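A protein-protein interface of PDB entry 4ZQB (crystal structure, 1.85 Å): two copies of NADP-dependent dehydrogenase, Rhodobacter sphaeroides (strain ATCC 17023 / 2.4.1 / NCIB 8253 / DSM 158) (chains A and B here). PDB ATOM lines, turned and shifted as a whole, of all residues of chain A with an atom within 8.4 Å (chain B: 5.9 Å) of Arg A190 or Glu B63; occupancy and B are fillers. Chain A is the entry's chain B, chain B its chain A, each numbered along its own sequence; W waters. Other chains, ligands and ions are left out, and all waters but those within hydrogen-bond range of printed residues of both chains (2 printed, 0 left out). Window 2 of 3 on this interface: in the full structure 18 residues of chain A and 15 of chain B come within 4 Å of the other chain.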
ATOM      1  N   HIS A 167      -6.506  -2.661 -26.244  1.00  0.00           N
ATOM      2  CA  HIS A 167      -6.717  -3.015 -24.865  1.00  0.00           C
ATOM      3  C   HIS A 167      -7.675  -4.203 -24.818  1.00  0.00           C
ATOM      4  O   HIS A 167      -8.673  -4.229 -25.550  1.00  0.00           O
ATOM      5  CB  HIS A 167      -7.321  -1.843 -24.113  1.00  0.00           C
ATOM      6  CG  HIS A 167      -6.368  -0.705 -23.940  1.00  0.00           C
ATOM      7  ND1 HIS A 167      -5.907  -0.299 -22.715  1.00  0.00           N
ATOM      8  CD2 HIS A 167      -5.731   0.067 -24.845  1.00  0.00           C
ATOM      9  CE1 HIS A 167      -5.078   0.721 -22.858  1.00  0.00           C
ATOM     10  NE2 HIS A 167      -4.947   0.958 -24.148  1.00  0.00           N
ATOM     11  N   TRP A 169      -9.844  -7.191 -22.342  1.00  0.00           N
ATOM     12  CA  TRP A 169     -10.450  -7.388 -21.041  1.00  0.00           C
ATOM     13  C   TRP A 169     -10.906  -8.849 -20.906  1.00  0.00           C
ATOM     14  O   TRP A 169     -11.552  -9.385 -21.809  1.00  0.00           O
ATOM     15  CB  TRP A 169     -11.668  -6.460 -20.860  1.00  0.00           C
ATOM     16  CG  TRP A 169     -12.319  -6.543 -19.521  1.00  0.00           C
ATOM     17  CD1 TRP A 169     -11.824  -6.071 -18.342  1.00  0.00           C
ATOM     18  CD2 TRP A 169     -13.580  -7.142 -19.214  1.00  0.00           C
ATOM     19  NE1 TRP A 169     -12.703  -6.332 -17.324  1.00  0.00           N
ATOM     20  CE2 TRP A 169     -13.794  -6.978 -17.830  1.00  0.00           C
ATOM     21  CE3 TRP A 169     -14.576  -7.755 -19.980  1.00  0.00           C
ATOM     22  CZ2 TRP A 169     -14.957  -7.420 -17.197  1.00  0.00           C
ATOM     23  CZ3 TRP A 169     -15.702  -8.201 -19.361  1.00  0.00           C
ATOM     24  CH2 TRP A 169     -15.900  -8.019 -17.974  1.00  0.00           C
ATOM     25  N   CYS A 181      -3.581  -5.535 -21.275  1.00  0.00           N
ATOM     26  CA  CYS A 181      -4.598  -6.456 -20.799  1.00  0.00           C
ATOM     27  C   CYS A 181      -5.120  -5.978 -19.451  1.00  0.00           C
ATOM     28  O   CYS A 181      -4.339  -5.571 -18.605  1.00  0.00           O
ATOM     29  CB  CYS A 181      -4.004  -7.841 -20.678  1.00  0.00           C
ATOM     30  SG  CYS A 181      -3.576  -8.522 -22.315  1.00  0.00           S
ATOM     31  N   HIS A 182      -6.430  -6.043 -19.267  1.00  0.00           N
ATOM     32  CA  HIS A 182      -7.131  -5.708 -18.020  1.00  0.00           C
ATOM     33  C   HIS A 182      -7.936  -6.907 -17.574  1.00  0.00           C
ATOM     34  O   HIS A 182      -8.425  -7.655 -18.404  1.00  0.00           O
ATOM     35  CB  HIS A 182      -8.101  -4.557 -18.289  1.00  0.00           C
ATOM     36  CG  HIS A 182      -7.409  -3.361 -18.836  1.00  0.00           C
ATOM     37  ND1 HIS A 182      -6.731  -2.465 -18.036  1.00  0.00           N
ATOM     38  CD2 HIS A 182      -7.246  -2.931 -20.101  1.00  0.00           C
ATOM     39  CE1 HIS A 182      -6.170  -1.537 -18.790  1.00  0.00           C
ATOM     40  NE2 HIS A 182      -6.461  -1.806 -20.045  1.00  0.00           N
ATOM     41  N   ALA A 183      -8.107  -7.066 -16.267  1.00  0.00           N
ATOM     42  CA  ALA A 183      -8.897  -8.188 -15.737  1.00  0.00           C
ATOM     43  C   ALA A 183      -9.846  -7.764 -14.624  1.00  0.00           C
ATOM     44  O   ALA A 183      -9.525  -6.876 -13.818  1.00  0.00           O
ATOM     45  CB  ALA A 183      -8.006  -9.319 -15.241  1.00  0.00           C
ATOM     46  N   GLY A 184     -10.999  -8.443 -14.603  1.00  0.00           N
ATOM     47  CA  GLY A 184     -11.959  -8.344 -13.528  1.00  0.00           C
ATOM     48  C   GLY A 184     -12.999  -7.262 -13.768  1.00  0.00           C
ATOM     49  O   GLY A 184     -12.760  -6.259 -14.467  1.00  0.00           O
ATOM     50  N   GLU A 185     -14.136  -7.457 -13.127  1.00  0.00           N
ATOM     51  CA  GLU A 185     -15.225  -6.509 -13.161  1.00  0.00           C
ATOM     52  C   GLU A 185     -14.735  -5.107 -12.781  1.00  0.00           C
ATOM     53  O   GLU A 185     -15.111  -4.144 -13.429  1.00  0.00           O
ATOM     54  CB  GLU A 185     -16.375  -6.944 -12.225  1.00  0.00           C
ATOM     55  CG  GLU A 185     -17.707  -6.246 -12.537  1.00  0.00           C
ATOM     56  CD  GLU A 185     -18.542  -6.983 -13.593  1.00  0.00           C
ATOM     57  OE1 GLU A 185     -17.956  -7.741 -14.412  1.00  0.00           O
ATOM     58  OE2 GLU A 185     -19.790  -6.801 -13.608  1.00  0.00           O
ATOM     59  N   GLU A 186     -13.869  -5.044 -11.767  1.00  0.00           N
ATOM     60  CA  GLU A 186     -13.346  -3.809 -11.213  1.00  0.00           C
ATOM     61  C   GLU A 186     -12.661  -2.871 -12.230  1.00  0.00           C
ATOM     62  O   GLU A 186     -12.606  -1.671 -11.992  1.00  0.00           O
ATOM     63  CB  GLU A 186     -12.428  -4.088  -9.993  1.00  0.00           C
ATOM     64  CG  GLU A 186     -11.365  -5.179 -10.165  1.00  0.00           C
ATOM     65  N   THR A 187     -12.150  -3.386 -13.355  1.00  0.00           N
ATOM     66  CA  THR A 187     -11.450  -2.539 -14.346  1.00  0.00           C
ATOM     67  C   THR A 187     -12.229  -2.205 -15.635  1.00  0.00           C
ATOM     68  O   THR A 187     -11.723  -1.462 -16.493  1.00  0.00           O
ATOM     69  CB  THR A 187     -10.102  -3.224 -14.754  1.00  0.00           C
ATOM     70  OG1 THR A 187     -10.363  -4.479 -15.397  1.00  0.00           O
ATOM     71  CG2 THR A 187      -9.226  -3.461 -13.534  1.00  0.00           C
ATOM     72  N   LEU A 188     -13.413  -2.791 -15.816  1.00  0.00           N
ATOM     73  CA  LEU A 188     -14.160  -2.667 -17.050  1.00  0.00           C
ATOM     74  C   LEU A 188     -14.542  -1.215 -17.400  1.00  0.00           C
ATOM     75  O   LEU A 188     -14.251  -0.752 -18.500  1.00  0.00           O
ATOM     76  CB  LEU A 188     -15.434  -3.531 -16.986  1.00  0.00           C
ATOM     77  CG  LEU A 188     -16.372  -3.432 -18.196  1.00  0.00           C
ATOM     78  CD1 LEU A 188     -15.656  -3.863 -19.453  1.00  0.00           C
ATOM     79  CD2 LEU A 188     -17.639  -4.230 -17.983  1.00  0.00           C
ATOM     80  N   GLU A 189     -15.225  -0.535 -16.476  1.00  0.00           N
ATOM     81  CA  GLU A 189     -15.711   0.826 -16.735  1.00  0.00           C
ATOM     82  C   GLU A 189     -14.558   1.799 -17.020  1.00  0.00           C
ATOM     83  O   GLU A 189     -14.684   2.668 -17.913  1.00  0.00           O
ATOM     84  CB  GLU A 189     -16.617   1.314 -15.606  1.00  0.00           C
ATOM     85  CG  GLU A 189     -17.921   0.524 -15.571  1.00  0.00           C
ATOM     86  CD  GLU A 189     -18.916   0.943 -14.496  1.00  0.00           C
ATOM     87  OE1 GLU A 189     -18.651   1.837 -13.713  1.00  0.00           O
ATOM     88  OE2 GLU A 189     -19.992   0.339 -14.414  1.00  0.00           O
ATOM     89  N   ARG A 190     -13.434   1.635 -16.325  1.00  0.00           N
ATOM     90  CA  ARG A 190     -12.236   2.458 -16.579  1.00  0.00           C
ATOM     91  C   ARG A 190     -11.733   2.206 -17.988  1.00  0.00           C
ATOM     92  O   ARG A 190     -11.447   3.153 -18.747  1.00  0.00           O
ATOM     93  CB  ARG A 190     -11.146   2.158 -15.554  1.00  0.00           C
ATOM     94  CG  ARG A 190      -9.987   3.149 -15.515  1.00  0.00           C
ATOM     95  CD  ARG A 190      -9.067   2.837 -14.335  1.00  0.00           C
ATOM     96  NE  ARG A 190      -8.538   1.458 -14.417  1.00  0.00           N
ATOM     97  CZ  ARG A 190      -7.737   0.888 -13.515  1.00  0.00           C
ATOM     98  NH1 ARG A 190      -7.392   1.543 -12.405  1.00  0.00           N
ATOM     99  NH2 ARG A 190      -7.257  -0.349 -13.737  1.00  0.00           N
ATOM    100  N   MET A 191     -11.632   0.922 -18.365  1.00  0.00           N
ATOM    101  CA  MET A 191     -11.198   0.545 -19.721  1.00  0.00           C
ATOM    102  C   MET A 191     -12.099   1.178 -20.793  1.00  0.00           C
ATOM    103  O   MET A 191     -11.601   1.711 -21.807  1.00  0.00           O
ATOM    104  CB  MET A 191     -11.108  -0.997 -19.925  1.00  0.00           C
ATOM    105  CG  MET A 191     -10.980  -1.380 -21.418  1.00  0.00           C
ATOM    106  SD  MET A 191     -10.579  -3.069 -21.964  1.00  0.00           S
ATOM    107  CE  MET A 191     -11.631  -3.174 -23.412  1.00  0.00           C
ATOM    108  N   LEU A 192     -13.396   1.074 -20.606  1.00  0.00           N
ATOM    109  CA  LEU A 192     -14.362   1.544 -21.596  1.00  0.00           C
ATOM    110  C   LEU A 192     -14.266   3.038 -21.829  1.00  0.00           C
ATOM    111  O   LEU A 192     -14.475   3.490 -22.949  1.00  0.00           O
ATOM    112  CB  LEU A 192     -15.791   1.166 -21.195  1.00  0.00           C
ATOM    113  CG  LEU A 192     -16.116  -0.327 -21.178  1.00  0.00           C
ATOM    114  CD1 LEU A 192     -17.522  -0.518 -20.592  1.00  0.00           C
ATOM    115  CD2 LEU A 192     -16.029  -0.955 -22.558  1.00  0.00           C
ATOM    116  N   GLY A 193     -13.933   3.786 -20.766  1.00  0.00           N
ATOM    117  CA  GLY A 193     -13.714   5.209 -20.850  1.00  0.00           C
ATOM    118  C   GLY A 193     -12.759   5.639 -21.926  1.00  0.00           C
ATOM    119  O   GLY A 193     -12.830   6.779 -22.406  1.00  0.00           O
ATOM    120  N   GLN A 194     -11.834   4.750 -22.282  1.00  0.00           N
ATOM    121  CA  GLN A 194     -10.815   5.031 -23.272  1.00  0.00           C
ATOM    122  C   GLN A 194     -11.092   4.513 -24.678  1.00  0.00           C
ATOM    123  O   GLN A 194     -10.320   4.805 -25.575  1.00  0.00           O
ATOM    124  CB  GLN A 194      -9.474   4.473 -22.778  1.00  0.00           C
ATOM    125  CG  GLN A 194      -8.976   5.182 -21.528  1.00  0.00           C
ATOM    126  CD  GLN A 194      -8.932   6.706 -21.720  1.00  0.00           C
ATOM    127  OE1 GLN A 194      -8.130   7.202 -22.515  1.00  0.00           O
ATOM    128  NE2 GLN A 194      -9.825   7.460 -21.023  1.00  0.00           N
ATOM    129  N   VAL A 195     -12.123   3.702 -24.863  1.00  0.00           N
ATOM    130  CA  VAL A 195     -12.255   2.856 -26.073  1.00  0.00           C
ATOM    131  C   VAL A 195     -13.041   3.553 -27.180  1.00  0.00           C
ATOM    132  O   VAL A 195     -14.172   3.938 -26.966  1.00  0.00           O
ATOM    133  CB  VAL A 195     -12.904   1.499 -25.719  1.00  0.00           C
ATOM    134  CG1 VAL A 195     -13.324   0.736 -26.964  1.00  0.00           C
ATOM    135  CG2 VAL A 195     -11.919   0.666 -24.926  1.00  0.00           C
ATOM    136  N   ARG A 216     -22.850   0.953 -18.640  1.00  0.00           N
ATOM    137  CA  ARG A 216     -21.573   0.635 -19.262  1.00  0.00           C
ATOM    138  C   ARG A 216     -21.414   1.331 -20.607  1.00  0.00           C
ATOM    139  O   ARG A 216     -20.319   1.813 -20.891  1.00  0.00           O
ATOM    140  CB  ARG A 216     -21.355  -0.867 -19.405  1.00  0.00           C
ATOM    141  CG  ARG A 216     -20.636  -1.518 -18.224  1.00  0.00           C
ATOM    142  CD  ARG A 216     -21.383  -1.428 -16.932  1.00  0.00           C
ATOM    143  NE  ARG A 216     -20.726  -2.133 -15.824  1.00  0.00           N
ATOM    144  CZ  ARG A 216     -20.881  -3.439 -15.519  1.00  0.00           C
ATOM    145  NH1 ARG A 216     -21.629  -4.239 -16.268  1.00  0.00           N
ATOM    146  NH2 ARG A 216     -20.259  -3.957 -14.461  1.00  0.00           N
ATOM    147  N   CYS A 219     -20.191   4.808 -20.311  1.00  0.00           N
ATOM    148  CA  CYS A 219     -18.748   4.929 -20.047  1.00  0.00           C
ATOM    149  C   CYS A 219     -17.942   5.213 -21.311  1.00  0.00           C
ATOM    150  O   CYS A 219     -16.862   5.789 -21.216  1.00  0.00           O
ATOM    151  CB  CYS A 219     -18.194   3.673 -19.333  1.00  0.00           C
ATOM    152  SG  CYS A 219     -18.862   3.482 -17.652  1.00  0.00           S
ATOM    153  N   LEU A 220     -18.440   4.810 -22.480  1.00  0.00           N
ATOM    154  CA  LEU A 220     -17.702   5.010 -23.715  1.00  0.00           C
ATOM    155  C   LEU A 220     -17.623   6.501 -24.045  1.00  0.00           C
ATOM    156  O   LEU A 220     -18.553   7.255 -23.741  1.00  0.00           O
ATOM    157  CB  LEU A 220     -18.326   4.224 -24.864  1.00  0.00           C
ATOM    158  CG  LEU A 220     -18.269   2.697 -24.772  1.00  0.00           C
ATOM    159  CD1 LEU A 220     -19.334   2.037 -25.619  1.00  0.00           C
ATOM    160  CD2 LEU A 220     -16.895   2.190 -25.181  1.00  0.00           C
ATOM    161  N   PRO A 221     -16.507   6.937 -24.658  1.00  0.00           N
ATOM    162  CA  PRO A 221     -16.451   8.301 -25.121  1.00  0.00           C
ATOM    163  C   PRO A 221     -17.452   8.601 -26.254  1.00  0.00           C
ATOM    164  O   PRO A 221     -17.864   7.711 -26.995  1.00  0.00           O
ATOM    165  CB  PRO A 221     -15.003   8.466 -25.608  1.00  0.00           C
ATOM    166  CG  PRO A 221     -14.550   7.089 -25.934  1.00  0.00           C
ATOM    167  CD  PRO A 221     -15.319   6.149 -25.058  1.00  0.00           C
ATOM    168  N   PHE B  37      -2.516  -2.340  -3.809  1.00  0.00           N
ATOM    169  CA  PHE B  37      -3.160  -1.197  -4.433  1.00  0.00           C
ATOM    170  C   PHE B  37      -4.662  -1.138  -4.161  1.00  0.00           C
ATOM    171  O   PHE B  37      -5.188  -0.075  -3.840  1.00  0.00           O
ATOM    172  CB  PHE B  37      -2.954  -1.213  -5.950  1.00  0.00           C
ATOM    173  CG  PHE B  37      -3.620  -0.062  -6.666  1.00  0.00           C
ATOM    174  CD1 PHE B  37      -2.992   1.173  -6.751  1.00  0.00           C
ATOM    175  CD2 PHE B  37      -4.883  -0.197  -7.238  1.00  0.00           C
ATOM    176  CE1 PHE B  37      -3.591   2.237  -7.426  1.00  0.00           C
ATOM    177  CE2 PHE B  37      -5.494   0.883  -7.894  1.00  0.00           C
ATOM    178  CZ  PHE B  37      -4.843   2.100  -7.989  1.00  0.00           C
ATOM    179  N   ARG B  45      -3.500   6.574  -1.628  1.00  0.00           N
ATOM    180  CA  ARG B  45      -2.824   6.510  -2.914  1.00  0.00           C
ATOM    181  C   ARG B  45      -1.915   7.715  -3.177  1.00  0.00           C
ATOM    182  O   ARG B  45      -0.838   7.556  -3.744  1.00  0.00           O
ATOM    183  CB  ARG B  45      -3.834   6.366  -4.057  1.00  0.00           C
ATOM    184  CG  ARG B  45      -4.374   4.959  -4.160  1.00  0.00           C
ATOM    185  CD  ARG B  45      -5.310   4.758  -5.306  1.00  0.00           C
ATOM    186  NE  ARG B  45      -5.769   3.366  -5.219  1.00  0.00           N
ATOM    187  CZ  ARG B  45      -7.038   2.950  -5.201  1.00  0.00           C
ATOM    188  NH1 ARG B  45      -8.052   3.809  -5.337  1.00  0.00           N
ATOM    189  NH2 ARG B  45      -7.280   1.654  -5.090  1.00  0.00           N
ATOM    190  N   ALA B  46      -2.334   8.883  -2.723  1.00  0.00           N
ATOM    191  CA  ALA B  46      -1.556  10.092  -2.879  1.00  0.00           C
ATOM    192  C   ALA B  46      -0.278  10.060  -2.025  1.00  0.00           C
ATOM    193  O   ALA B  46       0.643  10.797  -2.321  1.00  0.00           O
ATOM    194  CB  ALA B  46      -2.401  11.319  -2.569  1.00  0.00           C
ATOM    195  N   ASP B  57      -1.659  -3.652 -13.593  1.00  0.00           N
ATOM    196  CA  ASP B  57      -2.493  -2.883 -14.534  1.00  0.00           C
ATOM    197  C   ASP B  57      -1.915  -1.438 -14.615  1.00  0.00           C
ATOM    198  O   ASP B  57      -1.775  -0.774 -13.600  1.00  0.00           O
ATOM    199  CB  ASP B  57      -3.977  -2.925 -14.105  1.00  0.00           C
ATOM    200  CG  ASP B  57      -4.905  -2.268 -15.137  1.00  0.00           C
ATOM    201  OD1 ASP B  57      -4.527  -1.236 -15.740  1.00  0.00           O
ATOM    202  OD2 ASP B  57      -6.033  -2.762 -15.394  1.00  0.00           O
ATOM    203  N   PRO B  58      -1.487  -0.987 -15.812  1.00  0.00           N
ATOM    204  CA  PRO B  58      -0.883   0.368 -15.927  1.00  0.00           C
ATOM    205  C   PRO B  58      -1.797   1.486 -15.488  1.00  0.00           C
ATOM    206  O   PRO B  58      -1.310   2.514 -15.027  1.00  0.00           O
ATOM    207  CB  PRO B  58      -0.600   0.524 -17.423  1.00  0.00           C
ATOM    208  CG  PRO B  58      -1.308  -0.627 -18.095  1.00  0.00           C
ATOM    209  CD  PRO B  58      -1.482  -1.701 -17.097  1.00  0.00           C
ATOM    210  N   ALA B  59      -3.114   1.292 -15.614  1.00  0.00           N
ATOM    211  CA  ALA B  59      -4.047   2.311 -15.168  1.00  0.00           C
ATOM    212  C   ALA B  59      -4.004   2.523 -13.652  1.00  0.00           C
ATOM    213  O   ALA B  59      -4.343   3.610 -13.166  1.00  0.00           O
ATOM    214  CB  ALA B  59      -5.471   1.967 -15.612  1.00  0.00           C
ATOM    215  N   ASP B  60      -3.688   1.467 -12.896  1.00  0.00           N
ATOM    216  CA  ASP B  60      -3.532   1.594 -11.449  1.00  0.00           C
ATOM    217  C   ASP B  60      -2.336   2.488 -11.103  1.00  0.00           C
ATOM    218  O   ASP B  60      -2.429   3.353 -10.222  1.00  0.00           O
ATOM    219  CB  ASP B  60      -3.320   0.231 -10.791  1.00  0.00           C
ATOM    220  CG  ASP B  60      -4.577  -0.661 -10.818  1.00  0.00           C
ATOM    221  OD1 ASP B  60      -5.712  -0.196 -11.073  1.00  0.00           O
ATOM    222  OD2 ASP B  60      -4.399  -1.846 -10.506  1.00  0.00           O
ATOM    223  N   LEU B  61      -1.206   2.271 -11.775  1.00  0.00           N
ATOM    224  CA  LEU B  61      -0.028   3.126 -11.557  1.00  0.00           C
ATOM    225  C   LEU B  61      -0.291   4.582 -11.916  1.00  0.00           C
ATOM    226  O   LEU B  61       0.221   5.472 -11.250  1.00  0.00           O
ATOM    227  CB  LEU B  61       1.173   2.619 -12.340  1.00  0.00           C
ATOM    228  CG  LEU B  61       1.688   1.305 -11.745  1.00  0.00           C
ATOM    229  CD1 LEU B  61       2.542   0.613 -12.734  1.00  0.00           C
ATOM    230  CD2 LEU B  61       2.516   1.569 -10.497  1.00  0.00           C
ATOM    231  N   ALA B  62      -1.109   4.824 -12.942  1.00  0.00           N
ATOM    232  CA  ALA B  62      -1.494   6.186 -13.323  1.00  0.00           C
ATOM    233  C   ALA B  62      -2.322   6.905 -12.249  1.00  0.00           C
ATOM    234  O   ALA B  62      -2.466   8.140 -12.280  1.00  0.00           O
ATOM    235  CB  ALA B  62      -2.260   6.180 -14.628  1.00  0.00           C
ATOM    236  N   GLU B  63      -2.857   6.154 -11.297  1.00  0.00           N
ATOM    237  CA  GLU B  63      -3.591   6.704 -10.164  1.00  0.00           C
ATOM    238  C   GLU B  63      -2.719   6.867  -8.911  1.00  0.00           C
ATOM    239  O   GLU B  63      -3.245   7.029  -7.813  1.00  0.00           O
ATOM    240  CB  GLU B  63      -4.794   5.803  -9.861  1.00  0.00           C
ATOM    241  CG  GLU B  63      -5.807   5.769 -10.983  1.00  0.00           C
ATOM    242  CD  GLU B  63      -6.929   4.772 -10.765  1.00  0.00           C
ATOM    243  OE1 GLU B  63      -7.695   4.591 -11.722  1.00  0.00           O
ATOM    244  OE2 GLU B  63      -7.033   4.139  -9.678  1.00  0.00           O
ATOM    245  N   LEU B  64      -1.393   6.824  -9.067  1.00  0.00           N
ATOM    246  CA  LEU B  64      -0.464   7.142  -7.972  1.00  0.00           C
ATOM    247  C   LEU B  64       0.233   8.481  -8.316  1.00  0.00           C
ATOM    248  O   LEU B  64       1.335   8.488  -8.852  1.00  0.00           O
ATOM    249  CB  LEU B  64       0.540   6.011  -7.778  1.00  0.00           C
ATOM    250  CG  LEU B  64      -0.034   4.633  -7.394  1.00  0.00           C
ATOM    251  CD1 LEU B  64       1.106   3.600  -7.343  1.00  0.00           C
ATOM    252  CD2 LEU B  64      -0.783   4.621  -6.073  1.00  0.00           C
ATOM    253  N   PRO B  65      -0.432   9.607  -8.039  1.00  0.00           N
ATOM    254  CA  PRO B  65       0.018  10.917  -8.557  1.00  0.00           C
ATOM    255  C   PRO B  65       1.386  11.393  -8.081  1.00  0.00           C
ATOM    256  O   PRO B  65       2.064  12.132  -8.816  1.00  0.00           O
ATOM    257  CB  PRO B  65      -1.101  11.879  -8.091  1.00  0.00           C
ATOM    258  CG  PRO B  65      -1.625  11.240  -6.863  1.00  0.00           C
ATOM    259  CD  PRO B  65      -1.577   9.764  -7.123  1.00  0.00           C
HETATM  260  O   HOH W   1      -6.402  -5.332 -14.584  1.00  0.00           O
HETATM  261  O   HOH W   2      -8.323  -0.836 -10.105  1.00  0.00           O
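No position is printed for both chains.
Printed residues of chain B within 4 Å of His A182: Asp B57 (2.7 Å). Of the printed residues of chain B, Thr A187 touches Asp B57 (3.8 Å). Arg A190 touches just these residues of chain B: Asp B57, Ala B59, Asp B60 and Glu B63. Leu A220 touches none of the printed residues of chain B. Printed residues of chain A within 4 Å of Asp B57: His A182, Thr A187 and Arg A190. Printed residues of chain A within 4 Å of Ala B59: Arg A190. Of the printed residues of chain A, Asp B60 touches Arg A190 (2.8 Å). No residue of chain A comes within 4 Å of Ala B62. Glu B63 touches just one residue of chain A: Arg A190. The nearest residue of chain A that does not touch Glu B63 is Glu A186 (8.0 Å). The nearest printed residue of chain A that does not touch Ala B59 is His A182 (4.8 Å).
OD2 of Asp B57 lies within hydrogen-bond range of ND1 of His A182, 2.7 Å away. The guanidinium group (NH2) of Arg A190 lies within salt-bridge range of the side-chain carboxylate (OD2) of Asp B57, 3.2 Å away. The side-chain carboxylate (OD1) of Asp B60 lies within salt-bridge range of the guanidinium group (NH1) of Arg A190 (2.8 Å). The side-chain carboxylate (OE1) of Glu B63 is in salt-bridge range of the guanidinium group (NH1) of Arg A190, 3.1 Å away.
Water W1 lies within hydrogen-bond range of the side-chain carboxylate of Asp B57 (2.7 Å) and the backbone NH of Ala A183 (3.0 Å). Water W2 bridges OD1 of Asp B60 and NH1 of Arg A190.
N of Ala B59 is in hydrogen-bond range of OD1 of Asp B57, 2.9 Å away. A ring nitrogen (ND1) of His A167 is in hydrogen-bond range of a ring nitrogen (NE2) of His A182 (3.1 Å). O of Ala A183 lies within hydrogen-bond range of OG1 of Thr A187, at 3.0 Å. The side-chain hydroxyl (OG1) of Thr A187 lies within hydrogen-bond range of the backbone carbonyl oxygen (O) of Gly A184.
Hydrophobic or aromatic side chains of chain A within 4 Å of the printed part of chain B: His A182. Among the printed residues, Asp or Glu carboxylates within 4 Å of a Lys or Arg side-chain nitrogen of the other chain: Arg A190 with Asp B57 (3.2 Å), Arg A190 with Asp B60 (2.8 Å) and Arg A190 with Glu B63 (3.1 Å).
Among the printed residues, pairs that only touch across the chains: Thr A187 with Asp B57 and Arg A190 with Ala B59.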
